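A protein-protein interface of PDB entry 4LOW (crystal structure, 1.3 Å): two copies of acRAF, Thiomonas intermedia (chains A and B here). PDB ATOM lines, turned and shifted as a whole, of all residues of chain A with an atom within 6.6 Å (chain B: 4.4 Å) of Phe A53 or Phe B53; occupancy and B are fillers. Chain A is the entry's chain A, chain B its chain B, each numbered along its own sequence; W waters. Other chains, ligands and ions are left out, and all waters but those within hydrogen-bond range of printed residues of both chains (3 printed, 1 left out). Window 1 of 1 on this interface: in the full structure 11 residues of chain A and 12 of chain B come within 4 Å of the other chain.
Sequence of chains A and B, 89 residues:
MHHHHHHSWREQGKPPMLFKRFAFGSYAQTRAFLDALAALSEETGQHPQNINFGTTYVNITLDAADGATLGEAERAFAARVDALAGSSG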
ATOM      1  N   TYR A  27     -23.815   7.629  -3.513  1.00  0.00           N
ATOM      2  CA  TYR A  27     -23.629   6.242  -3.079  1.00  0.00           C
ATOM      3  C   TYR A  27     -22.511   5.578  -3.883  1.00  0.00           C
ATOM      4  O   TYR A  27     -21.687   4.879  -3.302  1.00  0.00           O
ATOM      5  CB  TYR A  27     -24.920   5.422  -3.245  1.00  0.00           C
ATOM      6  CG  TYR A  27     -24.727   3.958  -2.881  1.00  0.00           C
ATOM      7  CD1 TYR A  27     -24.698   3.552  -1.552  1.00  0.00           C
ATOM      8  CD2 TYR A  27     -24.441   3.003  -3.860  1.00  0.00           C
ATOM      9  CE1 TYR A  27     -24.445   2.222  -1.206  1.00  0.00           C
ATOM     10  CE2 TYR A  27     -24.197   1.671  -3.523  1.00  0.00           C
ATOM     11  CZ  TYR A  27     -24.182   1.294  -2.193  1.00  0.00           C
ATOM     12  OH  TYR A  27     -23.936   0.009  -1.807  1.00  0.00           O
ATOM     13  N   THR A  30     -19.189   6.552  -2.410  1.00  0.00           N
ATOM     14  CA  THR A  30     -19.002   5.974  -1.067  1.00  0.00           C
ATOM     15  C   THR A  30     -18.723   4.474  -1.167  1.00  0.00           C
ATOM     16  O   THR A  30     -17.826   3.955  -0.510  1.00  0.00           O
ATOM     17  CB  THR A  30     -20.292   6.164  -0.282  1.00  0.00           C
ATOM     18  OG1 THR A  30     -20.627   7.541  -0.292  1.00  0.00           O
ATOM     19  CG2 THR A  30     -20.178   5.691   1.157  1.00  0.00           C
ATOM     20  N   ARG A  31     -19.463   3.787  -2.051  1.00  0.00           N
ATOM     21  CA  ARG A  31     -19.302   2.339  -2.199  1.00  0.00           C
ATOM     22  C   ARG A  31     -17.952   1.988  -2.804  1.00  0.00           C
ATOM     23  O   ARG A  31     -17.333   1.006  -2.388  1.00  0.00           O
ATOM     24  CB  ARG A  31     -20.472   1.795  -3.023  1.00  0.00           C
ATOM     25  CG  ARG A  31     -20.567   0.298  -3.059  1.00  0.00           C
ATOM     26  CD  ARG A  31     -20.741  -0.285  -1.657  1.00  0.00           C
ATOM     27  NE  ARG A  31     -19.520  -0.877  -1.143  1.00  0.00           N
ATOM     28  CZ  ARG A  31     -19.425  -1.538  -0.001  1.00  0.00           C
ATOM     29  NH1 ARG A  31     -20.415  -1.485   0.892  1.00  0.00           N
ATOM     30  NH2 ARG A  31     -18.320  -2.202   0.288  1.00  0.00           N
ATOM     31  N   LEU A  34     -15.562   2.251   0.025  1.00  0.00           N
ATOM     32  CA  LEU A  34     -15.693   1.110   0.931  1.00  0.00           C
ATOM     33  C   LEU A  34     -15.087  -0.172   0.353  1.00  0.00           C
ATOM     34  O   LEU A  34     -14.407  -0.934   1.065  1.00  0.00           O
ATOM     35  CB  LEU A  34     -17.139   0.865   1.376  1.00  0.00           C
ATOM     36  CG  LEU A  34     -17.719   1.944   2.278  1.00  0.00           C
ATOM     37  CD1 LEU A  34     -19.236   1.839   2.293  1.00  0.00           C
ATOM     38  CD2 LEU A  34     -17.228   1.759   3.736  1.00  0.00           C
ATOM     39  N   LEU A  37     -11.336   0.171   0.529  1.00  0.00           N
ATOM     40  CA  LEU A  37     -10.886   0.072   1.905  1.00  0.00           C
ATOM     41  C   LEU A  37     -10.802  -1.393   2.297  1.00  0.00           C
ATOM     42  O   LEU A  37      -9.817  -1.784   2.981  1.00  0.00           O
ATOM     43  CB  LEU A  37     -11.857   0.907   2.779  1.00  0.00           C
ATOM     44  CG  LEU A  37     -11.661   0.925   4.294  1.00  0.00           C
ATOM     45  CD1 LEU A  37     -10.284   1.513   4.705  1.00  0.00           C
ATOM     46  CD2 LEU A  37     -12.737   1.740   4.972  1.00  0.00           C
ATOM     47  N   PRO A  48      -9.153  -1.536  10.502  1.00  0.00           N
ATOM     48  CA  PRO A  48      -9.623  -0.526  11.455  1.00  0.00           C
ATOM     49  C   PRO A  48     -10.352  -1.156  12.648  1.00  0.00           C
ATOM     50  O   PRO A  48     -10.991  -2.218  12.512  1.00  0.00           O
ATOM     51  CB  PRO A  48     -10.600   0.305  10.610  1.00  0.00           C
ATOM     52  CG  PRO A  48     -10.022   0.225   9.195  1.00  0.00           C
ATOM     53  CD  PRO A  48      -9.608  -1.244   9.134  1.00  0.00           C
ATOM     54  N   GLN A  49     -10.322  -0.460  13.778  1.00  0.00           N
ATOM     55  CA  GLN A  49     -11.096  -0.842  14.953  1.00  0.00           C
ATOM     56  C   GLN A  49     -12.591  -0.853  14.560  1.00  0.00           C
ATOM     57  O   GLN A  49     -13.332  -1.777  14.917  1.00  0.00           O
ATOM     58  CB  GLN A  49     -10.842   0.149  16.089  1.00  0.00           C
ATOM     59  CG  GLN A  49     -11.671  -0.125  17.348  1.00  0.00           C
ATOM     60  CD  GLN A  49     -11.456   0.913  18.394  1.00  0.00           C
ATOM     61  OE1 GLN A  49     -10.379   1.511  18.505  1.00  0.00           O
ATOM     62  NE2 GLN A  49     -12.466   1.104  19.220  1.00  0.00           N
ATOM     63  N   ASN A  50     -13.019   0.161  13.790  1.00  0.00           N
ATOM     64  CA  ASN A  50     -14.407   0.213  13.390  1.00  0.00           C
ATOM     65  C   ASN A  50     -14.565   1.082  12.170  1.00  0.00           C
ATOM     66  O   ASN A  50     -13.837   2.067  12.015  1.00  0.00           O
ATOM     67  CB  ASN A  50     -15.250   0.844  14.515  1.00  0.00           C
ATOM     68  CG  ASN A  50     -16.730   0.884  14.227  1.00  0.00           C
ATOM     69  OD1 ASN A  50     -17.207   1.896  13.694  1.00  0.00           O
ATOM     70  ND2 ASN A  50     -17.473  -0.163  14.518  1.00  0.00           N
ATOM     71  N   ILE A  51     -15.474   0.697  11.270  1.00  0.00           N
ATOM     72  CA  ILE A  51     -15.858   1.457  10.079  1.00  0.00           C
ATOM     73  C   ILE A  51     -17.348   1.662  10.207  1.00  0.00           C
ATOM     74  O   ILE A  51     -18.100   0.703  10.401  1.00  0.00           O
ATOM     75  CB  ILE A  51     -15.498   0.715   8.795  1.00  0.00           C
ATOM     76  CG1 ILE A  51     -13.991   0.587   8.643  1.00  0.00           C
ATOM     77  CG2 ILE A  51     -16.060   1.467   7.565  1.00  0.00           C
ATOM     78  CD1 ILE A  51     -13.569  -0.417   7.655  1.00  0.00           C
ATOM     79  N   ASN A  52     -17.814   2.900  10.121  1.00  0.00           N
ATOM     80  CA  ASN A  52     -19.171   3.280  10.424  1.00  0.00           C
ATOM     81  C   ASN A  52     -19.702   4.127   9.305  1.00  0.00           C
ATOM     82  O   ASN A  52     -19.164   5.224   9.123  1.00  0.00           O
ATOM     83  CB  ASN A  52     -19.083   4.035  11.774  1.00  0.00           C
ATOM     84  CG  ASN A  52     -20.277   4.798  12.203  1.00  0.00           C
ATOM     85  OD1 ASN A  52     -21.398   4.477  11.847  1.00  0.00           O
ATOM     86  ND2 ASN A  52     -20.048   5.750  13.116  1.00  0.00           N
ATOM     87  N   PHE A  53     -20.699   3.656   8.541  1.00  0.00           N
ATOM     88  CA  PHE A  53     -21.063   4.349   7.332  1.00  0.00           C
ATOM     89  C   PHE A  53     -22.512   4.461   7.086  1.00  0.00           C
ATOM     90  O   PHE A  53     -23.321   3.689   7.588  1.00  0.00           O
ATOM     91  CB  PHE A  53     -20.377   3.636   6.127  1.00  0.00           C
ATOM     92  CG  PHE A  53     -20.860   2.231   5.823  1.00  0.00           C
ATOM     93  CD1 PHE A  53     -20.262   1.131   6.418  1.00  0.00           C
ATOM     94  CD2 PHE A  53     -21.811   2.013   4.833  1.00  0.00           C
ATOM     95  CE1 PHE A  53     -20.693  -0.156   6.100  1.00  0.00           C
ATOM     96  CE2 PHE A  53     -22.206   0.730   4.483  1.00  0.00           C
ATOM     97  CZ  PHE A  53     -21.661  -0.342   5.126  1.00  0.00           C
ATOM     98  N   GLY A  54     -22.833   5.402   6.212  1.00  0.00           N
ATOM     99  CA  GLY A  54     -24.152   5.603   5.634  1.00  0.00           C
ATOM    100  C   GLY A  54     -24.021   5.617   4.127  1.00  0.00           C
ATOM    101  O   GLY A  54     -23.082   5.051   3.556  1.00  0.00           O
ATOM    102  N   THR A  55     -24.991   6.231   3.443  1.00  0.00           N
ATOM    103  CA  THR A  55     -24.905   6.230   1.960  1.00  0.00           C
ATOM    104  C   THR A  55     -23.907   7.225   1.420  1.00  0.00           C
ATOM    105  O   THR A  55     -23.431   7.049   0.298  1.00  0.00           O
ATOM    106  CB  THR A  55     -26.261   6.467   1.341  1.00  0.00           C
ATOM    107  OG1 THR A  55     -26.718   7.712   1.807  1.00  0.00           O
ATOM    108  CG2 THR A  55     -27.238   5.388   1.696  1.00  0.00           C
ATOM    109  N   THR A  56     -23.578   8.267   2.183  1.00  0.00           N
ATOM    110  CA  THR A  56     -22.741   9.378   1.685  1.00  0.00           C
ATOM    111  C   THR A  56     -21.568   9.686   2.596  1.00  0.00           C
ATOM    112  O   THR A  56     -20.871  10.682   2.385  1.00  0.00           O
ATOM    113  CB  THR A  56     -23.568  10.650   1.429  1.00  0.00           C
ATOM    114  OG1 THR A  56     -24.156  11.052   2.663  1.00  0.00           O
ATOM    115  CG2 THR A  56     -24.632  10.456   0.370  1.00  0.00           C
ATOM    116  N   TYR A  57     -21.240   8.800   3.550  1.00  0.00           N
ATOM    117  CA  TYR A  57     -20.136   9.096   4.441  1.00  0.00           C
ATOM    118  C   TYR A  57     -19.618   7.829   5.074  1.00  0.00           C
ATOM    119  O   TYR A  57     -20.367   6.827   5.196  1.00  0.00           O
ATOM    120  CB  TYR A  57     -20.539  10.122   5.557  1.00  0.00           C
ATOM    121  CG  TYR A  57     -21.771   9.730   6.317  1.00  0.00           C
ATOM    122  CD1 TYR A  57     -21.700   8.814   7.365  1.00  0.00           C
ATOM    123  CD2 TYR A  57     -23.032  10.188   5.933  1.00  0.00           C
ATOM    124  CE1 TYR A  57     -22.843   8.387   8.028  1.00  0.00           C
ATOM    125  CE2 TYR A  57     -24.187   9.754   6.590  1.00  0.00           C
ATOM    126  CZ  TYR A  57     -24.077   8.847   7.629  1.00  0.00           C
ATOM    127  OH  TYR A  57     -25.237   8.465   8.266  1.00  0.00           O
ATOM    128  N   VAL A  58     -18.366   7.880   5.508  1.00  0.00           N
ATOM    129  CA  VAL A  58     -17.710   6.747   6.148  1.00  0.00           C
ATOM    130  C   VAL A  58     -16.835   7.298   7.256  1.00  0.00           C
ATOM    131  O   VAL A  58     -15.987   8.169   7.005  1.00  0.00           O
ATOM    132  CB  VAL A  58     -16.816   5.978   5.134  1.00  0.00           C
ATOM    133  CG1 VAL A  58     -16.118   4.805   5.834  1.00  0.00           C
ATOM    134  CG2 VAL A  58     -17.607   5.496   3.926  1.00  0.00           C
ATOM    135  N   ASN A  59     -17.028   6.817   8.478  1.00  0.00           N
ATOM    136  CA  ASN A  59     -16.256   7.216   9.639  1.00  0.00           C
ATOM    137  C   ASN A  59     -15.323   6.076  10.019  1.00  0.00           C
ATOM    138  O   ASN A  59     -15.794   4.951  10.240  1.00  0.00           O
ATOM    139  CB  ASN A  59     -17.205   7.446  10.803  1.00  0.00           C
ATOM    140  CG  ASN A  59     -18.235   8.512  10.525  1.00  0.00           C
ATOM    141  OD1 ASN A  59     -17.924   9.706  10.407  1.00  0.00           O
ATOM    142  ND2 ASN A  59     -19.512   8.110  10.476  1.00  0.00           N
ATOM    143  N   ARG B  31     -16.735 -10.041   6.170  1.00  0.00           N
ATOM    144  CA  ARG B  31     -16.612  -9.432   4.871  1.00  0.00           C
ATOM    145  C   ARG B  31     -17.629 -10.039   3.869  1.00  0.00           C
ATOM    146  O   ARG B  31     -18.232  -9.313   3.074  1.00  0.00           O
ATOM    147  CB  ARG B  31     -15.157  -9.582   4.377  1.00  0.00           C
ATOM    148  CG  ARG B  31     -14.877  -8.947   3.024  1.00  0.00           C
ATOM    149  CD  ARG B  31     -15.036  -7.429   3.133  1.00  0.00           C
ATOM    150  NE  ARG B  31     -16.316  -6.956   2.619  1.00  0.00           N
ATOM    151  CZ  ARG B  31     -16.795  -5.718   2.793  1.00  0.00           C
ATOM    152  NH1 ARG B  31     -16.147  -4.844   3.571  1.00  0.00           N
ATOM    153  NH2 ARG B  31     -17.906  -5.344   2.174  1.00  0.00           N
ATOM    154  N   LEU B  34     -21.003  -8.639   4.711  1.00  0.00           N
ATOM    155  CA  LEU B  34     -21.121  -7.232   4.298  1.00  0.00           C
ATOM    156  C   LEU B  34     -21.279  -7.082   2.784  1.00  0.00           C
ATOM    157  O   LEU B  34     -22.023  -6.201   2.331  1.00  0.00           O
ATOM    158  CB  LEU B  34     -19.886  -6.443   4.747  1.00  0.00           C
ATOM    159  CG  LEU B  34     -19.811  -6.161   6.245  1.00  0.00           C
ATOM    160  CD1 LEU B  34     -18.430  -5.745   6.618  1.00  0.00           C
ATOM    161  CD2 LEU B  34     -20.807  -5.039   6.628  1.00  0.00           C
ATOM    162  N   ASN B  50     -27.781   3.079   9.325  1.00  0.00           N
ATOM    163  CA  ASN B  50     -26.399   2.977   9.747  1.00  0.00           C
ATOM    164  C   ASN B  50     -25.947   1.566   9.687  1.00  0.00           C
ATOM    165  O   ASN B  50     -26.708   0.662  10.075  1.00  0.00           O
ATOM    166  CB  ASN B  50     -26.237   3.435  11.215  1.00  0.00           C
ATOM    167  CG  ASN B  50     -24.800   3.337  11.664  1.00  0.00           C
ATOM    168  OD1 ASN B  50     -24.385   2.437  12.407  1.00  0.00           O
ATOM    169  ND2 ASN B  50     -24.004   4.238  11.150  1.00  0.00           N
ATOM    170  N   ILE B  51     -24.671   1.386   9.304  1.00  0.00           N
ATOM    171  CA  ILE B  51     -23.967   0.109   9.392  1.00  0.00           C
ATOM    172  C   ILE B  51     -22.621   0.403   9.987  1.00  0.00           C
ATOM    173  O   ILE B  51     -21.936   1.320   9.523  1.00  0.00           O
ATOM    174  CB  ILE B  51     -23.796  -0.594   8.050  1.00  0.00           C
ATOM    175  CG1 ILE B  51     -25.169  -0.904   7.426  1.00  0.00           C
ATOM    176  CG2 ILE B  51     -22.983  -1.899   8.239  1.00  0.00           C
ATOM    177  CD1 ILE B  51     -25.102  -1.251   5.989  1.00  0.00           C
ATOM    178  N   ASN B  52     -22.219  -0.316  11.026  1.00  0.00           N
ATOM    179  CA  ASN B  52     -20.844  -0.134  11.500  1.00  0.00           C
ATOM    180  C   ASN B  52     -20.305  -1.500  11.864  1.00  0.00           C
ATOM    181  O   ASN B  52     -21.089  -2.374  12.303  1.00  0.00           O
ATOM    182  CB  ASN B  52     -20.666   0.904  12.598  1.00  0.00           C
ATOM    183  CG  ASN B  52     -21.224   0.490  13.888  1.00  0.00           C
ATOM    184  OD1 ASN B  52     -20.562  -0.249  14.642  1.00  0.00           O
ATOM    185  ND2 ASN B  52     -22.418   0.978  14.207  1.00  0.00           N
ATOM    186  N   PHE B  53     -19.017  -1.721  11.617  1.00  0.00           N
ATOM    187  CA  PHE B  53     -18.476  -3.053  11.752  1.00  0.00           C
ATOM    188  C   PHE B  53     -17.026  -3.064  12.129  1.00  0.00           C
ATOM    189  O   PHE B  53     -16.274  -2.100  11.929  1.00  0.00           O
ATOM    190  CB  PHE B  53     -18.650  -3.813  10.405  1.00  0.00           C
ATOM    191  CG  PHE B  53     -17.820  -3.270   9.246  1.00  0.00           C
ATOM    192  CD1 PHE B  53     -16.577  -3.809   8.952  1.00  0.00           C
ATOM    193  CD2 PHE B  53     -18.329  -2.296   8.394  1.00  0.00           C
ATOM    194  CE1 PHE B  53     -15.845  -3.378   7.848  1.00  0.00           C
ATOM    195  CE2 PHE B  53     -17.593  -1.877   7.281  1.00  0.00           C
ATOM    196  CZ  PHE B  53     -16.356  -2.421   7.022  1.00  0.00           C
ATOM    197  N   GLY B  54     -16.662  -4.195  12.725  1.00  0.00           N
ATOM    198  CA  GLY B  54     -15.299  -4.543  13.074  1.00  0.00           C
ATOM    199  C   GLY B  54     -14.932  -5.858  12.420  1.00  0.00           C
ATOM    200  O   GLY B  54     -15.626  -6.314  11.509  1.00  0.00           O
ATOM    201  N   TYR B  57     -18.020  -8.391  13.732  1.00  0.00           N
ATOM    202  CA  TYR B  57     -19.384  -8.004  14.028  1.00  0.00           C
ATOM    203  C   TYR B  57     -19.825  -6.940  13.032  1.00  0.00           C
ATOM    204  O   TYR B  57     -18.991  -6.217  12.470  1.00  0.00           O
ATOM    205  CB  TYR B  57     -19.554  -7.445  15.460  1.00  0.00           C
ATOM    206  CG  TYR B  57     -18.804  -6.151  15.686  1.00  0.00           C
ATOM    207  CD1 TYR B  57     -19.393  -4.923  15.399  1.00  0.00           C
ATOM    208  CD2 TYR B  57     -17.477  -6.157  16.098  1.00  0.00           C
ATOM    209  CE1 TYR B  57     -18.678  -3.734  15.524  1.00  0.00           C
ATOM    210  CE2 TYR B  57     -16.759  -4.972  16.243  1.00  0.00           C
ATOM    211  CZ  TYR B  57     -17.364  -3.767  15.940  1.00  0.00           C
ATOM    212  OH  TYR B  57     -16.687  -2.578  16.051  1.00  0.00           O
ATOM    213  N   VAL B  58     -21.141  -6.860  12.857  1.00  0.00           N
ATOM    214  CA  VAL B  58     -21.791  -5.835  12.037  1.00  0.00           C
ATOM    215  C   VAL B  58     -23.011  -5.363  12.803  1.00  0.00           C
ATOM    216  O   VAL B  58     -23.910  -6.162  13.080  1.00  0.00           O
ATOM    217  CB  VAL B  58     -22.227  -6.326  10.643  1.00  0.00           C
ATOM    218  CG1 VAL B  58     -22.823  -5.157   9.838  1.00  0.00           C
ATOM    219  CG2 VAL B  58     -21.050  -6.934   9.888  1.00  0.00           C
HETATM  220  O   HOH W   1     -13.439  -2.359  10.871  1.00  0.00           O
HETATM  221  O   HOH W   2     -25.544   6.381   9.768  1.00  0.00           O
HETATM  222  O   HOH W   3     -14.324  -2.725  17.251  1.00  0.00           O
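N of Phe A53 lies within hydrogen-bond range of O of Ile B51 (2.8 Å).
The side-chain amide nitrogen (ND2) of Asn A50 lies close to the backbone carbonyl oxygen (O) of Phe B53, at 3.4 Å.
O of Ile A51 lies within hydrogen-bond range of N of Phe B53 (2.9 Å).
The side-chain amide nitrogen (ND2) of Asn B50 sits at hydrogen-bond distance from the side-chain amide oxygen (OD1) of Asn A52 (2.7 Å).
ND2 of Asn A50 sits at hydrogen-bond distance from OH of Tyr B57 (3.0 Å).
The side-chain amide oxygen (OD1) of Asn B52 sits at hydrogen-bond distance from the side-chain amide nitrogen (ND2) of Asn A50, 3.1 Å away.
The side-chain amide oxygen (OD1) of Asn B50 sits at hydrogen-bond distance from the side-chain amide nitrogen (ND2) of Asn B52 (3.0 Å).
The backbone NH (N) of Asn A59 sits at hydrogen-bond distance from the backbone carbonyl oxygen (O) of Asn A52 (2.7 Å).
Water W2 bridges OH of Tyr A57 and ND2 of Asn B50.
Water W3 lies within hydrogen-bond range of the side-chain hydroxyl of Tyr B57 and the backbone carbonyl oxygen of Gln A49.
Water W1 lies within hydrogen-bond range of O of Pro A48 (3.0 Å) and O of Phe B53 (3.0 Å).
Arg A31 touches its own counterpart, Arg B31.
Asn A50 touches Phe B53, and with the chains exchanged Phe A53 touches Asn B50.
Ile A51 touches Phe B53, and with the chains exchanged Phe A53 touches Ile B51.
Phe A53 touches its own counterpart, Phe B53.
Positions printed for both chains: 31, 34, 50, 51, 52, 53, 54, 57 and 58.
Of the 15 pairs that touch across the chains among the printed residues, 12 have their exchanged pair printed and touching as well.
Of the 9 printed residues of chain B, 7 touch a printed residue of chain A.
Hydrophobic or aromatic side chains of chain B that line the printed part of chain A: Ile B51, Phe B53 and Tyr B57.
Hydrophobic or aromatic side chains of chain A that line the printed part of chain B: Ile A51 and Phe A53.
Leu A37 touches none of the printed residues of chain B.
Printed residues of chain B within 4 Å of Asn A50: Asn B52, Phe B53 and Tyr B57.
Printed residues of chain B within 4 Å of Ile A51: Ile B51, Asn B52 and Phe B53.
Of chain B, only Asn B50, Ile B51 and Phe B53 come within 4 Å of Phe A53.
Gly A54 touches none of the printed residues of chain B.
Of the printed residues of chain A, Ile B51 touches Ile A51 (3.98 Å), Asn A52 (3.5 Å) and Phe A53 (2.8 Å).
Of chain A, only Asn A50 (3.3 Å), Ile A51 (2.9 Å) and Phe A53 (3.7 Å) come within 4 Å of Phe B53.
Of the printed residues of chain A, Gly B54 touches Gln A49 (3.9 Å).
The nearest printed residue of chain B that does not touch Phe A53 is Asn B52 (4.8 Å).
The nearest residue of chain A that does not touch Phe B53 is Gln A49 (4.2 Å).
Among the printed residues, merely in contact across the chains: Arg A31 with Arg B31, Gln A49 with Gly B54, Gln A49 with Tyr B57, Ile A51 with Ile B51, Ile A51 with Asn B52, Asn A52 with Ile B51, Asn A52 with Asn B52, Phe A53 with Asn B50 and Phe A53 with Phe B53.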
